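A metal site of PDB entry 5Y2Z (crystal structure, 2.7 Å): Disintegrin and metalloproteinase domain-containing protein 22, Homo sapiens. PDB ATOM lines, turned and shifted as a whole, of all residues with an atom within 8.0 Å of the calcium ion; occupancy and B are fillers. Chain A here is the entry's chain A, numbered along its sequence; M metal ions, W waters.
The backbone carbonyl oxygen (O) of Asp 93 is in hydrogen-bond range of the backbone NH (N) of Cys 117 (3.2 Å).
The backbone NH of Ala 94 is in hydrogen-bond range of the backbone carbonyl oxygen of Glu 10 (3.3 Å).
The side-chain sulfur of Cys 201 forms a disulfide with the side-chain sulfur of Cys 117 (2.0 Å).
The calcium ion is bound by the side-chain amide nitrogen (ND2) of Asn 204, the side-chain carboxylate (OD2) of Asp 93, the side-chain carboxylate (OE2) of Glu 10, the side-chain carboxylate (OD1) of Asp 93, water W1, the backbone carbonyl oxygen (O) of Cys 201, the side-chain amide oxygen (OD1) of Asn 204 and water W2.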
ATOM      1  N   TYR A   8       5.382 -11.460   5.834  1.00  0.00           N
ATOM      2  CA  TYR A   8       4.945 -11.294   4.455  1.00  0.00           C
ATOM      3  C   TYR A   8       5.413 -12.420   3.554  1.00  0.00           C
ATOM      4  O   TYR A   8       6.617 -12.653   3.402  1.00  0.00           O
ATOM      5  CB  TYR A   8       5.444  -9.959   3.904  1.00  0.00           C
ATOM      6  CG  TYR A   8       4.998  -8.754   4.690  1.00  0.00           C
ATOM      7  CD1 TYR A   8       5.723  -8.310   5.795  1.00  0.00           C
ATOM      8  CD2 TYR A   8       3.863  -8.032   4.313  1.00  0.00           C
ATOM      9  CE1 TYR A   8       5.321  -7.216   6.507  1.00  0.00           C
ATOM     10  CE2 TYR A   8       3.467  -6.925   5.027  1.00  0.00           C
ATOM     11  CZ  TYR A   8       4.197  -6.514   6.130  1.00  0.00           C
ATOM     12  OH  TYR A   8       3.809  -5.419   6.848  1.00  0.00           O
ATOM     13  N   ILE A   9       4.465 -13.139   2.965  1.00  0.00           N
ATOM     14  CA  ILE A   9       4.784 -14.181   2.006  1.00  0.00           C
ATOM     15  C   ILE A   9       4.718 -13.680   0.572  1.00  0.00           C
ATOM     16  O   ILE A   9       3.641 -13.531  -0.002  1.00  0.00           O
ATOM     17  CB  ILE A   9       3.826 -15.382   2.152  1.00  0.00           C
ATOM     18  CG1 ILE A   9       3.913 -15.953   3.575  1.00  0.00           C
ATOM     19  CG2 ILE A   9       4.144 -16.463   1.133  1.00  0.00           C
ATOM     20  CD1 ILE A   9       2.960 -17.097   3.819  1.00  0.00           C
ATOM     21  N   GLU A  10       5.899 -13.421   0.004  1.00  0.00           N
ATOM     22  CA  GLU A  10       6.011 -13.044  -1.390  1.00  0.00           C
ATOM     23  C   GLU A  10       5.769 -14.268  -2.258  1.00  0.00           C
ATOM     24  O   GLU A  10       6.651 -15.099  -2.409  1.00  0.00           O
ATOM     25  CB  GLU A  10       7.392 -12.420  -1.685  1.00  0.00           C
ATOM     26  CG  GLU A  10       7.706 -11.166  -0.870  1.00  0.00           C
ATOM     27  CD  GLU A  10       9.036 -10.517  -1.270  1.00  0.00           C
ATOM     28  OE1 GLU A  10       9.010  -9.351  -1.711  1.00  0.00           O
ATOM     29  OE2 GLU A  10      10.090 -11.181  -1.127  1.00  0.00           O
ATOM     30  N   LEU A  11       4.560 -14.367  -2.808  1.00  0.00           N
ATOM     31  CA  LEU A  11       4.143 -15.568  -3.502  1.00  0.00           C
ATOM     32  C   LEU A  11       4.169 -15.411  -5.029  1.00  0.00           C
ATOM     33  O   LEU A  11       3.770 -14.371  -5.569  1.00  0.00           O
ATOM     34  CB  LEU A  11       2.737 -15.974  -3.050  1.00  0.00           C
ATOM     35  CG  LEU A  11       2.087 -17.198  -3.696  1.00  0.00           C
ATOM     36  CD1 LEU A  11       2.833 -18.485  -3.356  1.00  0.00           C
ATOM     37  CD2 LEU A  11       0.625 -17.304  -3.316  1.00  0.00           C
ATOM     38  N   VAL A  56       3.563 -11.484  -5.991  1.00  0.00           N
ATOM     39  CA  VAL A  56       4.693 -10.696  -6.474  1.00  0.00           C
ATOM     40  C   VAL A  56       5.076 -11.045  -7.902  1.00  0.00           C
ATOM     41  O   VAL A  56       5.719 -10.264  -8.584  1.00  0.00           O
ATOM     42  CB  VAL A  56       5.939 -10.873  -5.575  1.00  0.00           C
ATOM     43  CG1 VAL A  56       5.674 -10.323  -4.181  1.00  0.00           C
ATOM     44  CG2 VAL A  56       6.345 -12.335  -5.510  1.00  0.00           C
ATOM     45  N   LYS A  91      12.313 -13.595  -8.249  1.00  0.00           N
ATOM     46  CA  LYS A  91      12.479 -13.800  -6.819  1.00  0.00           C
ATOM     47  C   LYS A  91      11.144 -13.881  -6.085  1.00  0.00           C
ATOM     48  O   LYS A  91      10.240 -13.070  -6.319  1.00  0.00           O
ATOM     49  CB  LYS A  91      13.341 -12.665  -6.246  1.00  0.00           C
ATOM     50  CG  LYS A  91      14.753 -12.617  -6.820  1.00  0.00           C
ATOM     51  CD  LYS A  91      15.480 -13.937  -6.611  1.00  0.00           C
ATOM     52  CE  LYS A  91      16.891 -13.905  -7.178  1.00  0.00           C
ATOM     53  NZ  LYS A  91      17.578 -15.216  -6.967  1.00  0.00           N
ATOM     54  N   SER A  92      11.031 -14.866  -5.200  1.00  0.00           N
ATOM     55  CA  SER A  92       9.824 -15.053  -4.404  1.00  0.00           C
ATOM     56  C   SER A  92      10.099 -15.935  -3.187  1.00  0.00           C
ATOM     57  O   SER A  92      11.003 -16.751  -3.190  1.00  0.00           O
ATOM     58  CB  SER A  92       8.729 -15.683  -5.263  1.00  0.00           C
ATOM     59  OG  SER A  92       9.112 -16.985  -5.679  1.00  0.00           O
ATOM     60  N   ASP A  93       9.306 -15.745  -2.135  1.00  0.00           N
ATOM     61  CA  ASP A  93       9.488 -16.519  -0.914  1.00  0.00           C
ATOM     62  C   ASP A  93       8.917 -17.938  -1.111  1.00  0.00           C
ATOM     63  O   ASP A  93       9.336 -18.884  -0.443  1.00  0.00           O
ATOM     64  CB  ASP A  93       8.826 -15.822   0.294  1.00  0.00           C
ATOM     65  CG  ASP A  93       9.396 -14.421   0.592  1.00  0.00           C
ATOM     66  OD1 ASP A  93      10.604 -14.165   0.388  1.00  0.00           O
ATOM     67  OD2 ASP A  93       8.622 -13.550   1.030  1.00  0.00           O
ATOM     68  N   ALA A  94       7.957 -18.064  -2.030  1.00  0.00           N
ATOM     69  CA  ALA A  94       7.384 -19.375  -2.367  1.00  0.00           C
ATOM     70  C   ALA A  94       6.753 -19.372  -3.766  1.00  0.00           C
ATOM     71  O   ALA A  94       6.174 -18.369  -4.197  1.00  0.00           O
ATOM     72  CB  ALA A  94       6.345 -19.781  -1.332  1.00  0.00           C
ATOM     73  N   CYS A 117      11.368 -19.876   1.798  1.00  0.00           N
ATOM     74  CA  CYS A 117      12.706 -19.285   1.694  1.00  0.00           C
ATOM     75  C   CYS A 117      13.708 -20.217   1.005  1.00  0.00           C
ATOM     76  O   CYS A 117      14.858 -19.846   0.812  1.00  0.00           O
ATOM     77  CB  CYS A 117      13.212 -18.888   3.080  1.00  0.00           C
ATOM     78  SG  CYS A 117      12.018 -17.911   4.031  1.00  0.00           S
ATOM     79  N   GLY A 199      11.575 -19.186   8.259  1.00  0.00           N
ATOM     80  CA  GLY A 199      10.847 -18.047   7.717  1.00  0.00           C
ATOM     81  C   GLY A 199      11.618 -16.742   7.767  1.00  0.00           C
ATOM     82  O   GLY A 199      11.028 -15.694   8.057  1.00  0.00           O
ATOM     83  N   ALA A 200      12.909 -16.789   7.476  1.00  0.00           N
ATOM     84  CA  ALA A 200      13.746 -15.585   7.492  1.00  0.00           C
ATOM     85  C   ALA A 200      13.405 -14.609   6.366  1.00  0.00           C
ATOM     86  O   ALA A 200      13.515 -13.394   6.532  1.00  0.00           O
ATOM     87  CB  ALA A 200      15.214 -15.969   7.420  1.00  0.00           C
ATOM     88  N   CYS A 201      12.986 -15.137   5.221  1.00  0.00           N
ATOM     89  CA  CYS A 201      12.695 -14.300   4.056  1.00  0.00           C
ATOM     90  C   CYS A 201      11.306 -13.656   4.112  1.00  0.00           C
ATOM     91  O   CYS A 201      10.832 -13.062   3.133  1.00  0.00           O
ATOM     92  CB  CYS A 201      12.803 -15.143   2.780  1.00  0.00           C
ATOM     93  SG  CYS A 201      11.564 -16.448   2.689  1.00  0.00           S
ATOM     94  N   LEU A 202      10.667 -13.772   5.263  1.00  0.00           N
ATOM     95  CA  LEU A 202       9.277 -13.338   5.428  1.00  0.00           C
ATOM     96  C   LEU A 202       9.142 -11.964   6.076  1.00  0.00           C
ATOM     97  O   LEU A 202       8.037 -11.545   6.413  1.00  0.00           O
ATOM     98  CB  LEU A 202       8.508 -14.366   6.251  1.00  0.00           C
ATOM     99  CG  LEU A 202       7.727 -15.466   5.528  1.00  0.00           C
ATOM    100  CD1 LEU A 202       8.444 -15.935   4.283  1.00  0.00           C
ATOM    101  CD2 LEU A 202       7.527 -16.615   6.488  1.00  0.00           C
ATOM    102  N   PHE A 203      10.266 -11.275   6.252  1.00  0.00           N
ATOM    103  CA  PHE A 203      10.262 -10.037   7.021  1.00  0.00           C
ATOM    104  C   PHE A 203      10.550  -8.798   6.174  1.00  0.00           C
ATOM    105  O   PHE A 203      10.635  -7.695   6.696  1.00  0.00           O
ATOM    106  CB  PHE A 203      11.240 -10.159   8.180  1.00  0.00           C
ATOM    107  CG  PHE A 203      10.797 -11.161   9.215  1.00  0.00           C
ATOM    108  CD1 PHE A 203      11.114 -12.504   9.082  1.00  0.00           C
ATOM    109  CD2 PHE A 203      10.051 -10.764  10.310  1.00  0.00           C
ATOM    110  CE1 PHE A 203      10.704 -13.425  10.031  1.00  0.00           C
ATOM    111  CE2 PHE A 203       9.638 -11.677  11.262  1.00  0.00           C
ATOM    112  CZ  PHE A 203       9.959 -13.012  11.118  1.00  0.00           C
ATOM    113  N   ASN A 204      10.689  -8.995   4.858  1.00  0.00           N
ATOM    114  CA  ASN A 204      10.729  -7.896   3.909  1.00  0.00           C
ATOM    115  C   ASN A 204       9.306  -7.504   3.497  1.00  0.00           C
ATOM    116  O   ASN A 204       8.549  -8.337   3.004  1.00  0.00           O
ATOM    117  CB  ASN A 204      11.560  -8.260   2.673  1.00  0.00           C
ATOM    118  CG  ASN A 204      11.207  -9.631   2.101  1.00  0.00           C
ATOM    119  OD1 ASN A 204      11.668 -10.647   2.615  1.00  0.00           O
ATOM    120  ND2 ASN A 204      10.426  -9.654   1.036  1.00  0.00           N
ATOM    121  N   LYS A 205       8.956  -6.241   3.716  1.00  0.00           N
ATOM    122  CA  LYS A 205       7.603  -5.788   3.393  1.00  0.00           C
ATOM    123  C   LYS A 205       7.541  -5.295   1.954  1.00  0.00           C
ATOM    124  O   LYS A 205       8.249  -4.359   1.584  1.00  0.00           O
ATOM    125  CB  LYS A 205       7.154  -4.684   4.348  1.00  0.00           C
ATOM    126  CG  LYS A 205       5.743  -4.197   4.079  1.00  0.00           C
ATOM    127  CD  LYS A 205       5.361  -3.057   5.010  1.00  0.00           C
ATOM    128  CE  LYS A 205       3.978  -2.528   4.680  1.00  0.00           C
ATOM    129  NZ  LYS A 205       3.544  -1.477   5.633  1.00  0.00           N
ATOM    130  N   PRO A 206       6.702  -5.952   1.137  1.00  0.00           N
ATOM    131  CA  PRO A 206       6.493  -5.563  -0.269  1.00  0.00           C
ATOM    132  C   PRO A 206       5.913  -4.162  -0.377  1.00  0.00           C
ATOM    133  O   PRO A 206       5.151  -3.744   0.508  1.00  0.00           O
ATOM    134  CB  PRO A 206       5.500  -6.611  -0.777  1.00  0.00           C
ATOM    135  CG  PRO A 206       5.620  -7.762   0.174  1.00  0.00           C
ATOM    136  CD  PRO A 206       5.923  -7.142   1.496  1.00  0.00           C
HETATM  137 CA    CA M   1      10.326 -11.922   1.107  1.00  0.00          CA
HETATM  138  O   HOH W   1      12.482 -12.492   0.290  1.00  0.00           O
HETATM  139  O   HOH W   2       8.142 -11.108   2.636  1.00  0.00           O
